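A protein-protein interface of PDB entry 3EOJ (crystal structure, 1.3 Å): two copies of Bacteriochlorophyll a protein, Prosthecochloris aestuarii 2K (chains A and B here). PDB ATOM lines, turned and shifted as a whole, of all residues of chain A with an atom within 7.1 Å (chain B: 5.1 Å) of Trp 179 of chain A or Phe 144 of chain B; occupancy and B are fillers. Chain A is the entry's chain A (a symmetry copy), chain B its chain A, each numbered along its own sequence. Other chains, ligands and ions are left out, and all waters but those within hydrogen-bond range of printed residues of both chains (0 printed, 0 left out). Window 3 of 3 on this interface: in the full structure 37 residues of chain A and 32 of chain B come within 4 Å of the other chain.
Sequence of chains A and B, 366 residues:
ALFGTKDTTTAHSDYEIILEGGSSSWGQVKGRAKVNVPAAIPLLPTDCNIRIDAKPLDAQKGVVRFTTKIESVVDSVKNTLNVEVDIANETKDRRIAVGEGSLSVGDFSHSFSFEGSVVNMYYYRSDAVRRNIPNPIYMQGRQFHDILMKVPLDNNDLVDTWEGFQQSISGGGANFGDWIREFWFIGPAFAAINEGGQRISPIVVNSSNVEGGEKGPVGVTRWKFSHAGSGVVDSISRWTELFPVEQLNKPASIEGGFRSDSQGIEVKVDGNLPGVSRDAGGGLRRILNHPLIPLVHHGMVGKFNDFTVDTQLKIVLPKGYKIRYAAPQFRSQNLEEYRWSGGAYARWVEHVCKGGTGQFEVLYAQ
OH of Tyr 123 of chain B sits at hydrogen-bond distance from OE2 of Glu 182 of chain A.
The guanidinium group (NH2) of Arg 142 of chain B is in salt-bridge range of the side-chain carboxylate (OE2) of Glu 182 of chain A (2.9 Å).
The side-chain carboxylate (OD1) of Asp 178 of chain A is in salt-bridge range of the guanidinium group (NH1) of Arg 199 of chain B, at 2.9 Å.
The guanidinium group (NH1) of Arg 199 of chain B lies within salt-bridge range of the side-chain carboxylate (OE1) of Glu 182 of chain A (2.8 Å).
NE1 of Trp 179 of chain A sits close to NE of Arg 142 of chain B (3.4 Å).
The backbone carbonyl oxygen (O) of Val 119 of chain B is in hydrogen-bond range of the backbone NH (N) of Phe 144 of chain B (2.8 Å).
The backbone NH (N) of Met 121 of chain B is in hydrogen-bond range of the backbone carbonyl oxygen (O) of Arg 142 of chain B.
The guanidinium group of Arg 142 of chain B sits at hydrogen-bond distance from the side-chain hydroxyl of Tyr 123 of chain B (3.1 Å).
OG of Ser 226 of chain B sits at hydrogen-bond distance from NH1 of Arg 142 of chain B (2.9 Å).
OD1 of Asp 178 of chain A is in salt-bridge range of NH2 of Arg 181 of chain A, at 2.8 Å.
CB of Trp 179 of chain A touches OH of Tyr 123 of chain B (3.3 Å).
Phe 144 of chain B touches Trp 179 of chain A.
NH2 of Arg 199 of chain B touches NH2 of Arg 181 of chain A, 3.9 Å away.
CB of Tyr 123 of chain B touches CD1 of Phe 183 of chain A, at 3.99 Å.
Phe 190 of chain A touches Arg 199 of chain B (CZ to CD, 3.8 Å).
Gly 177 of chain A touches none of the printed residues of chain B.
Of the printed residues of chain B, Asp 178 of chain A touches Arg 199.
Printed residues of chain B within 4 Å of Trp 179 of chain A: Tyr 123 (3.3 Å), Arg 142 (3.2 Å) and Phe 144 (3.8 Å).
Of the printed residues of chain B, Glu 182 of chain A touches Tyr 123 (2.4 Å), Arg 142 (2.9 Å) and Arg 199 (2.8 Å).
Of the printed residues of chain B, Phe 183 of chain A touches Tyr 123 (3.99 Å).
Phe 144 of chain B touches one residue of chain A.
Of the printed residues of chain A, Arg 199 of chain B touches Asp 178 (2.9 Å), Arg 181 (3.9 Å), Glu 182 (2.8 Å) and Phe 190 (3.8 Å).
The nearest residue of chain A that does not touch Phe 144 of chain B is Asn 175 of chain A (6.6 Å).
The nearest printed residue of chain A that does not touch Arg 142 of chain B is Asp 178 of chain A (5.4 Å).
Of the 14 printed residues of chain B, 4 touch a printed residue of chain A.
Printed residues of chain B that touch a printed residue of chain A: Tyr 123, Arg 142, Phe 144 and Arg 199.
Of the 15 printed residues of chain A, 6 touch a printed residue of chain B.
Printed residues of chain A that touch a printed residue of chain B: Asp 178, Trp 179, Arg 181, Glu 182, Phe 183 and Phe 190.
Hydrophobic or aromatic side chains of chain A that line the printed part of chain B: Trp 179, Phe 183 and Phe 190.
Among the printed residues, 10 pairs touch across the chains.
No position is printed for both chains.
Of the 10 pairs that touch across the chains among the printed residues, none has its exchanged pair printed and touching as well.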
ATOM      1  N   SER A 168      34.666  -8.313 -27.974  1.00  0.00           N
ATOM      2  CA  SER A 168      33.971  -9.591 -27.913  1.00  0.00           C
ATOM      3  C   SER A 168      34.671 -10.487 -26.904  1.00  0.00           C
ATOM      4  O   SER A 168      34.006 -11.187 -26.133  1.00  0.00           O
ATOM      5  CB  SER A 168      33.930 -10.291 -29.266  1.00  0.00           C
ATOM      6  OG  SER A 168      33.121  -9.575 -30.174  1.00  0.00           O
ATOM      7  N   GLY A 172      35.162 -11.483 -22.336  1.00  0.00           N
ATOM      8  CA  GLY A 172      34.309 -12.631 -22.384  1.00  0.00           C
ATOM      9  C   GLY A 172      34.853 -13.903 -21.779  1.00  0.00           C
ATOM     10  O   GLY A 172      34.138 -14.865 -21.997  1.00  0.00           O
ATOM     11  N   ALA A 174      35.743 -17.566 -20.642  1.00  0.00           N
ATOM     12  CA  ALA A 174      35.431 -18.762 -21.419  1.00  0.00           C
ATOM     13  C   ALA A 174      34.288 -18.621 -22.384  1.00  0.00           C
ATOM     14  O   ALA A 174      34.136 -19.405 -23.352  1.00  0.00           O
ATOM     15  CB  ALA A 174      35.173 -19.971 -20.513  1.00  0.00           C
ATOM     16  N   ASN A 175      33.395 -17.631 -22.145  1.00  0.00           N
ATOM     17  CA  ASN A 175      32.247 -17.554 -23.059  1.00  0.00           C
ATOM     18  C   ASN A 175      32.678 -17.294 -24.480  1.00  0.00           C
ATOM     19  O   ASN A 175      32.065 -17.830 -25.382  1.00  0.00           O
ATOM     20  CB  ASN A 175      31.302 -16.437 -22.598  1.00  0.00           C
ATOM     21  CG  ASN A 175      30.581 -16.824 -21.305  1.00  0.00           C
ATOM     22  OD1 ASN A 175      30.388 -17.993 -20.917  1.00  0.00           O
ATOM     23  ND2 ASN A 175      30.164 -15.767 -20.620  1.00  0.00           N
ATOM     24  N   PHE A 176      33.711 -16.489 -24.680  1.00  0.00           N
ATOM     25  CA  PHE A 176      34.096 -16.139 -26.064  1.00  0.00           C
ATOM     26  C   PHE A 176      34.328 -17.378 -26.899  1.00  0.00           C
ATOM     27  O   PHE A 176      33.769 -17.530 -27.987  1.00  0.00           O
ATOM     28  CB  PHE A 176      35.354 -15.273 -26.044  1.00  0.00           C
ATOM     29  CG  PHE A 176      35.877 -15.098 -27.444  1.00  0.00           C
ATOM     30  CD1 PHE A 176      35.267 -14.181 -28.279  1.00  0.00           C
ATOM     31  CD2 PHE A 176      36.912 -15.857 -27.913  1.00  0.00           C
ATOM     32  CE1 PHE A 176      35.676 -14.030 -29.578  1.00  0.00           C
ATOM     33  CE2 PHE A 176      37.335 -15.711 -29.241  1.00  0.00           C
ATOM     34  CZ  PHE A 176      36.712 -14.803 -30.071  1.00  0.00           C
ATOM     35  N   GLY A 177      35.167 -18.288 -26.389  1.00  0.00           N
ATOM     36  CA  GLY A 177      35.596 -19.426 -27.170  1.00  0.00           C
ATOM     37  C   GLY A 177      34.549 -20.544 -27.209  1.00  0.00           C
ATOM     38  O   GLY A 177      34.663 -21.476 -28.018  1.00  0.00           O
ATOM     39  N   ASP A 178      33.550 -20.448 -26.358  1.00  0.00           N
ATOM     40  CA  ASP A 178      32.411 -21.355 -26.335  1.00  0.00           C
ATOM     41  C   ASP A 178      31.388 -20.932 -27.386  1.00  0.00           C
ATOM     42  O   ASP A 178      31.049 -21.649 -28.350  1.00  0.00           O
ATOM     43  CB  ASP A 178      31.861 -21.378 -24.921  1.00  0.00           C
ATOM     44  CG  ASP A 178      30.550 -22.123 -24.727  1.00  0.00           C
ATOM     45  OD1 ASP A 178      30.053 -22.756 -25.658  1.00  0.00           O
ATOM     46  OD2 ASP A 178      30.007 -22.045 -23.588  1.00  0.00           O
ATOM     47  N   TRP A 179      30.896 -19.697 -27.225  1.00  0.00           N
ATOM     48  CA  TRP A 179      29.826 -19.109 -28.052  1.00  0.00           C
ATOM     49  C   TRP A 179      30.254 -18.808 -29.480  1.00  0.00           C
ATOM     50  O   TRP A 179      29.425 -18.621 -30.359  1.00  0.00           O
ATOM     51  CB  TRP A 179      29.375 -17.828 -27.367  1.00  0.00           C
ATOM     52  CG  TRP A 179      28.774 -18.009 -26.013  1.00  0.00           C
ATOM     53  CD1 TRP A 179      28.420 -19.160 -25.372  1.00  0.00           C
ATOM     54  CD2 TRP A 179      28.433 -16.932 -25.122  1.00  0.00           C
ATOM     55  NE1 TRP A 179      27.887 -18.856 -24.148  1.00  0.00           N
ATOM     56  CE2 TRP A 179      27.896 -17.496 -23.967  1.00  0.00           C
ATOM     57  CE3 TRP A 179      28.561 -15.546 -25.187  1.00  0.00           C
ATOM     58  CZ2 TRP A 179      27.460 -16.753 -22.883  1.00  0.00           C
ATOM     59  CZ3 TRP A 179      28.138 -14.775 -24.116  1.00  0.00           C
ATOM     60  CH2 TRP A 179      27.599 -15.387 -22.969  1.00  0.00           C
ATOM     61  N   ILE A 180      31.593 -18.768 -29.720  1.00  0.00           N
ATOM     62  CA  ILE A 180      32.047 -18.543 -31.098  1.00  0.00           C
ATOM     63  C   ILE A 180      31.574 -19.659 -32.014  1.00  0.00           C
ATOM     64  O   ILE A 180      31.477 -19.475 -33.212  1.00  0.00           O
ATOM     65  CB  ILE A 180      33.573 -18.365 -31.116  1.00  0.00           C
ATOM     66  CG1 ILE A 180      34.092 -17.734 -32.405  1.00  0.00           C
ATOM     67  CG2 ILE A 180      34.328 -19.666 -30.820  1.00  0.00           C
ATOM     68  CD1 ILE A 180      33.685 -16.310 -32.654  1.00  0.00           C
ATOM     69  N   ARG A 181      31.278 -20.851 -31.497  1.00  0.00           N
ATOM     70  CA  ARG A 181      30.974 -21.992 -32.340  1.00  0.00           C
ATOM     71  C   ARG A 181      29.690 -21.801 -33.145  1.00  0.00           C
ATOM     72  O   ARG A 181      29.658 -22.176 -34.327  1.00  0.00           O
ATOM     73  CB  ARG A 181      30.959 -23.277 -31.491  1.00  0.00           C
ATOM     74  CG  ARG A 181      32.394 -23.642 -31.048  1.00  0.00           C
ATOM     75  CD  ARG A 181      32.489 -24.851 -30.135  1.00  0.00           C
ATOM     76  NE  ARG A 181      31.964 -24.491 -28.814  1.00  0.00           N
ATOM     77  CZ  ARG A 181      31.897 -25.363 -27.816  1.00  0.00           C
ATOM     78  NH1 ARG A 181      32.340 -26.593 -28.013  1.00  0.00           N
ATOM     79  NH2 ARG A 181      31.404 -24.996 -26.655  1.00  0.00           N
ATOM     80  N   GLU A 182      28.662 -21.178 -32.550  1.00  0.00           N
ATOM     81  CA  GLU A 182      27.428 -20.940 -33.319  1.00  0.00           C
ATOM     82  C   GLU A 182      27.557 -19.731 -34.241  1.00  0.00           C
ATOM     83  O   GLU A 182      26.751 -19.579 -35.164  1.00  0.00           O
ATOM     84  CB  GLU A 182      26.221 -20.818 -32.392  1.00  0.00           C
ATOM     85  CG  GLU A 182      26.298 -19.695 -31.356  1.00  0.00           C
ATOM     86  CD  GLU A 182      26.818 -20.118 -30.021  1.00  0.00           C
ATOM     87  OE1 GLU A 182      27.546 -21.132 -29.933  1.00  0.00           O
ATOM     88  OE2 GLU A 182      26.507 -19.424 -29.007  1.00  0.00           O
ATOM     89  N   PHE A 183      28.567 -18.872 -34.048  1.00  0.00           N
ATOM     90  CA  PHE A 183      28.920 -17.844 -35.049  1.00  0.00           C
ATOM     91  C   PHE A 183      29.602 -18.477 -36.258  1.00  0.00           C
ATOM     92  O   PHE A 183      29.259 -18.225 -37.413  1.00  0.00           O
ATOM     93  CB  PHE A 183      29.843 -16.804 -34.386  1.00  0.00           C
ATOM     94  CG  PHE A 183      30.398 -15.797 -35.361  1.00  0.00           C
ATOM     95  CD1 PHE A 183      29.556 -14.782 -35.859  1.00  0.00           C
ATOM     96  CD2 PHE A 183      31.699 -15.855 -35.788  1.00  0.00           C
ATOM     97  CE1 PHE A 183      29.976 -13.829 -36.751  1.00  0.00           C
ATOM     98  CE2 PHE A 183      32.143 -14.865 -36.705  1.00  0.00           C
ATOM     99  CZ  PHE A 183      31.284 -13.899 -37.178  1.00  0.00           C
ATOM    100  N   TRP A 184      30.608 -19.290 -35.962  1.00  0.00           N
ATOM    101  CA  TRP A 184      31.478 -19.982 -36.932  1.00  0.00           C
ATOM    102  C   TRP A 184      30.695 -20.911 -37.851  1.00  0.00           C
ATOM    103  O   TRP A 184      30.815 -20.856 -39.071  1.00  0.00           O
ATOM    104  CB  TRP A 184      32.533 -20.703 -36.111  1.00  0.00           C
ATOM    105  CG  TRP A 184      33.575 -21.529 -36.774  1.00  0.00           C
ATOM    106  CD1 TRP A 184      33.834 -21.800 -38.090  1.00  0.00           C
ATOM    107  CD2 TRP A 184      34.560 -22.250 -36.032  1.00  0.00           C
ATOM    108  NE1 TRP A 184      34.916 -22.625 -38.216  1.00  0.00           N
ATOM    109  CE2 TRP A 184      35.375 -22.930 -36.941  1.00  0.00           C
ATOM    110  CE3 TRP A 184      34.818 -22.406 -34.649  1.00  0.00           C
ATOM    111  CZ2 TRP A 184      36.441 -23.740 -36.545  1.00  0.00           C
ATOM    112  CZ3 TRP A 184      35.855 -23.200 -34.238  1.00  0.00           C
ATOM    113  CH2 TRP A 184      36.644 -23.853 -35.193  1.00  0.00           C
ATOM    114  N   PHE A 190      25.847 -25.736 -38.008  1.00  0.00           N
ATOM    115  CA  PHE A 190      25.997 -26.117 -36.606  1.00  0.00           C
ATOM    116  C   PHE A 190      25.393 -27.503 -36.361  1.00  0.00           C
ATOM    117  O   PHE A 190      26.058 -28.359 -35.769  1.00  0.00           O
ATOM    118  CB  PHE A 190      25.347 -25.069 -35.713  1.00  0.00           C
ATOM    119  CG  PHE A 190      25.660 -25.274 -34.250  1.00  0.00           C
ATOM    120  CD1 PHE A 190      26.741 -24.630 -33.663  1.00  0.00           C
ATOM    121  CD2 PHE A 190      24.857 -26.093 -33.459  1.00  0.00           C
ATOM    122  CE1 PHE A 190      27.014 -24.803 -32.330  1.00  0.00           C
ATOM    123  CE2 PHE A 190      25.158 -26.258 -32.114  1.00  0.00           C
ATOM    124  CZ  PHE A 190      26.233 -25.609 -31.532  1.00  0.00           C
ATOM    125  N   PRO A 202      35.837 -25.776 -27.794  1.00  0.00           N
ATOM    126  CA  PRO A 202      35.976 -24.318 -27.697  1.00  0.00           C
ATOM    127  C   PRO A 202      37.274 -23.852 -28.319  1.00  0.00           C
ATOM    128  O   PRO A 202      38.278 -24.595 -28.341  1.00  0.00           O
ATOM    129  CB  PRO A 202      35.954 -24.025 -26.187  1.00  0.00           C
ATOM    130  CG  PRO A 202      35.216 -25.201 -25.613  1.00  0.00           C
ATOM    131  CD  PRO A 202      35.668 -26.383 -26.466  1.00  0.00           C
ATOM    132  N   SER B 117      13.083  -9.393 -18.482  1.00  0.00           N
ATOM    133  CA  SER B 117      13.824  -8.656 -19.469  1.00  0.00           C
ATOM    134  C   SER B 117      14.497  -9.691 -20.386  1.00  0.00           C
ATOM    135  O   SER B 117      14.949 -10.726 -19.921  1.00  0.00           O
ATOM    136  CB  SER B 117      14.831  -7.728 -18.834  1.00  0.00           C
ATOM    137  OG  SER B 117      15.564  -6.813 -19.630  1.00  0.00           O
ATOM    138  N   VAL B 118      14.518  -9.359 -21.670  1.00  0.00           N
ATOM    139  CA  VAL B 118      15.225 -10.179 -22.664  1.00  0.00           C
ATOM    140  C   VAL B 118      16.102  -9.254 -23.497  1.00  0.00           C
ATOM    141  O   VAL B 118      15.599  -8.228 -23.977  1.00  0.00           O
ATOM    142  CB  VAL B 118      14.243 -10.959 -23.541  1.00  0.00           C
ATOM    143  CG1 VAL B 118      14.993 -11.736 -24.616  1.00  0.00           C
ATOM    144  CG2 VAL B 118      13.390 -11.903 -22.713  1.00  0.00           C
ATOM    145  N   VAL B 119      17.368  -9.625 -23.595  1.00  0.00           N
ATOM    146  CA  VAL B 119      18.345  -8.862 -24.381  1.00  0.00           C
ATOM    147  C   VAL B 119      18.831  -9.705 -25.522  1.00  0.00           C
ATOM    148  O   VAL B 119      19.448 -10.745 -25.285  1.00  0.00           O
ATOM    149  CB  VAL B 119      19.504  -8.350 -23.503  1.00  0.00           C
ATOM    150  CG1 VAL B 119      20.548  -7.649 -24.391  1.00  0.00           C
ATOM    151  CG2 VAL B 119      18.999  -7.435 -22.405  1.00  0.00           C
ATOM    152  N   ASN B 120      18.559  -9.282 -26.736  1.00  0.00           N
ATOM    153  CA  ASN B 120      19.089  -9.957 -27.929  1.00  0.00           C
ATOM    154  C   ASN B 120      20.463  -9.382 -28.282  1.00  0.00           C
ATOM    155  O   ASN B 120      20.589  -8.157 -28.313  1.00  0.00           O
ATOM    156  CB  ASN B 120      18.128  -9.812 -29.105  1.00  0.00           C
ATOM    157  CG  ASN B 120      18.395 -10.803 -30.206  1.00  0.00           C
ATOM    158  OD1 ASN B 120      18.177 -12.000 -30.025  1.00  0.00           O
ATOM    159  ND2 ASN B 120      18.860 -10.338 -31.362  1.00  0.00           N
ATOM    160  N   MET B 121      21.439 -10.237 -28.540  1.00  0.00           N
ATOM    161  CA  MET B 121      22.807  -9.807 -28.841  1.00  0.00           C
ATOM    162  C   MET B 121      23.296 -10.555 -30.082  1.00  0.00           C
ATOM    163  O   MET B 121      23.648 -11.748 -30.012  1.00  0.00           O
ATOM    164  CB  MET B 121      23.742 -10.001 -27.645  1.00  0.00           C
ATOM    165  CG  MET B 121      24.997  -9.165 -27.559  1.00  0.00           C
ATOM    166  SD  MET B 121      25.856  -9.046 -25.962  1.00  0.00           S
ATOM    167  CE  MET B 121      24.814  -7.793 -25.177  1.00  0.00           C
ATOM    168  N   TYR B 123      26.175 -11.583 -32.613  1.00  0.00           N
ATOM    169  CA  TYR B 123      27.596 -11.667 -32.252  1.00  0.00           C
ATOM    170  C   TYR B 123      28.496 -10.657 -32.954  1.00  0.00           C
ATOM    171  O   TYR B 123      29.600 -10.320 -32.517  1.00  0.00           O
ATOM    172  CB  TYR B 123      28.102 -13.076 -32.559  1.00  0.00           C
ATOM    173  CG  TYR B 123      27.628 -14.140 -31.606  1.00  0.00           C
ATOM    174  CD1 TYR B 123      28.222 -14.211 -30.345  1.00  0.00           C
ATOM    175  CD2 TYR B 123      26.647 -15.067 -31.912  1.00  0.00           C
ATOM    176  CE1 TYR B 123      27.841 -15.163 -29.419  1.00  0.00           C
ATOM    177  CE2 TYR B 123      26.257 -16.039 -30.991  1.00  0.00           C
ATOM    178  CZ  TYR B 123      26.859 -16.078 -29.744  1.00  0.00           C
ATOM    179  OH  TYR B 123      26.514 -17.026 -28.800  1.00  0.00           O
ATOM    180  N   ARG B 142      22.882 -14.500 -29.430  1.00  0.00           N
ATOM    181  CA  ARG B 142      22.513 -15.058 -28.141  1.00  0.00           C
ATOM    182  C   ARG B 142      21.522 -14.110 -27.455  1.00  0.00           C
ATOM    183  O   ARG B 142      21.656 -12.874 -27.616  1.00  0.00           O
ATOM    184  CB  ARG B 142      23.762 -15.301 -27.287  1.00  0.00           C
ATOM    185  CG  ARG B 142      23.522 -15.944 -25.919  1.00  0.00           C
ATOM    186  CD  ARG B 142      24.787 -16.517 -25.312  1.00  0.00           C
ATOM    187  NE  ARG B 142      25.277 -17.720 -25.998  1.00  0.00           N
ATOM    188  CZ  ARG B 142      24.993 -18.975 -25.691  1.00  0.00           C
ATOM    189  NH1 ARG B 142      24.168 -19.252 -24.682  1.00  0.00           N
ATOM    190  NH2 ARG B 142      25.498 -19.975 -26.355  1.00  0.00           N
ATOM    191  N   GLN B 143      20.565 -14.677 -26.726  1.00  0.00           N
ATOM    192  CA  GLN B 143      19.420 -13.910 -26.246  1.00  0.00           C
ATOM    193  C   GLN B 143      19.209 -14.256 -24.771  1.00  0.00           C
ATOM    194  O   GLN B 143      18.892 -15.393 -24.403  1.00  0.00           O
ATOM    195  CB  GLN B 143      18.229 -14.236 -27.093  1.00  0.00           C
ATOM    196  CG  GLN B 143      16.954 -13.473 -26.751  1.00  0.00           C
ATOM    197  CD  GLN B 143      15.818 -13.913 -27.672  1.00  0.00           C
ATOM    198  OE1 GLN B 143      14.923 -14.624 -27.242  1.00  0.00           O
ATOM    199  NE2 GLN B 143      15.955 -13.430 -28.915  1.00  0.00           N
ATOM    200  N   PHE B 144      19.448 -13.233 -23.921  1.00  0.00           N
ATOM    201  CA  PHE B 144      19.580 -13.376 -22.482  1.00  0.00           C
ATOM    202  C   PHE B 144      18.247 -13.074 -21.797  1.00  0.00           C
ATOM    203  O   PHE B 144      17.741 -11.956 -21.918  1.00  0.00           O
ATOM    204  CB  PHE B 144      20.662 -12.435 -21.942  1.00  0.00           C
ATOM    205  CG  PHE B 144      22.012 -12.707 -22.559  1.00  0.00           C
ATOM    206  CD1 PHE B 144      22.895 -13.579 -21.957  1.00  0.00           C
ATOM    207  CD2 PHE B 144      22.414 -12.100 -23.748  1.00  0.00           C
ATOM    208  CE1 PHE B 144      24.123 -13.867 -22.511  1.00  0.00           C
ATOM    209  CE2 PHE B 144      23.648 -12.385 -24.282  1.00  0.00           C
ATOM    210  CZ  PHE B 144      24.522 -13.255 -23.676  1.00  0.00           C
ATOM    211  N   HIS B 145      17.696 -14.065 -21.098  1.00  0.00           N
ATOM    212  CA  HIS B 145      16.477 -13.907 -20.318  1.00  0.00           C
ATOM    213  C   HIS B 145      16.776 -13.726 -18.834  1.00  0.00           C
ATOM    214  O   HIS B 145      17.603 -14.467 -18.282  1.00  0.00           O
ATOM    215  CB  HIS B 145      15.660 -15.176 -20.445  1.00  0.00           C
ATOM    216  CG  HIS B 145      14.907 -15.357 -21.723  1.00  0.00           C
ATOM    217  ND1 HIS B 145      15.484 -15.378 -22.998  1.00  0.00           N
ATOM    218  CD2 HIS B 145      13.590 -15.557 -21.930  1.00  0.00           C
ATOM    219  CE1 HIS B 145      14.513 -15.585 -23.910  1.00  0.00           C
ATOM    220  NE2 HIS B 145      13.344 -15.687 -23.294  1.00  0.00           N
ATOM    221  N   ASP B 146      16.074 -12.793 -18.219  1.00  0.00           N
ATOM    222  CA  ASP B 146      16.142 -12.564 -16.775  1.00  0.00           C
ATOM    223  C   ASP B 146      14.697 -12.517 -16.283  1.00  0.00           C
ATOM    224  O   ASP B 146      13.940 -11.687 -16.764  1.00  0.00           O
ATOM    225  CB  ASP B 146      16.930 -11.269 -16.498  1.00  0.00           C
ATOM    226  CG  ASP B 146      17.250 -11.076 -15.022  1.00  0.00           C
ATOM    227  OD1 ASP B 146      16.985 -11.996 -14.233  1.00  0.00           O
ATOM    228  OD2 ASP B 146      17.797  -9.976 -14.721  1.00  0.00           O
ATOM    229  N   ARG B 199      20.964 -23.419 -29.076  1.00  0.00           N
ATOM    230  CA  ARG B 199      21.603 -23.820 -27.837  1.00  0.00           C
ATOM    231  C   ARG B 199      20.787 -23.214 -26.672  1.00  0.00           C
ATOM    232  O   ARG B 199      20.378 -22.051 -26.744  1.00  0.00           O
ATOM    233  CB  ARG B 199      23.017 -23.342 -27.732  1.00  0.00           C
ATOM    234  CG  ARG B 199      23.887 -23.729 -28.936  1.00  0.00           C
ATOM    235  CD  ARG B 199      25.317 -23.177 -28.808  1.00  0.00           C
ATOM    236  NE  ARG B 199      25.968 -23.857 -27.685  1.00  0.00           N
ATOM    237  CZ  ARG B 199      27.126 -23.583 -27.150  1.00  0.00           C
ATOM    238  NH1 ARG B 199      27.883 -22.605 -27.625  1.00  0.00           N
ATOM    239  NH2 ARG B 199      27.582 -24.292 -26.128  1.00  0.00           N
ATOM    240  N   PHE B 225      18.623 -17.536 -17.983  1.00  0.00           N
ATOM    241  CA  PHE B 225      19.201 -18.429 -18.964  1.00  0.00           C
ATOM    242  C   PHE B 225      19.408 -17.624 -20.236  1.00  0.00           C
ATOM    243  O   PHE B 225      18.798 -16.540 -20.392  1.00  0.00           O
ATOM    244  CB  PHE B 225      18.352 -19.658 -19.296  1.00  0.00           C
ATOM    245  CG  PHE B 225      17.128 -19.412 -20.158  1.00  0.00           C
ATOM    246  CD1 PHE B 225      17.198 -19.692 -21.537  1.00  0.00           C
ATOM    247  CD2 PHE B 225      15.958 -18.889 -19.641  1.00  0.00           C
ATOM    248  CE1 PHE B 225      16.091 -19.472 -22.335  1.00  0.00           C
ATOM    249  CE2 PHE B 225      14.860 -18.677 -20.461  1.00  0.00           C
ATOM    250  CZ  PHE B 225      14.918 -18.950 -21.812  1.00  0.00           C
ATOM    251  N   SER B 226      20.214 -18.135 -21.146  1.00  0.00           N
ATOM    252  CA  SER B 226      20.257 -17.598 -22.497  1.00  0.00           C
ATOM    253  C   SER B 226      20.030 -18.747 -23.481  1.00  0.00           C
ATOM    254  O   SER B 226      20.297 -19.890 -23.194  1.00  0.00           O
ATOM    255  CB  SER B 226      21.559 -16.859 -22.759  1.00  0.00           C
ATOM    256  OG  SER B 226      22.688 -17.713 -22.756  1.00  0.00           O
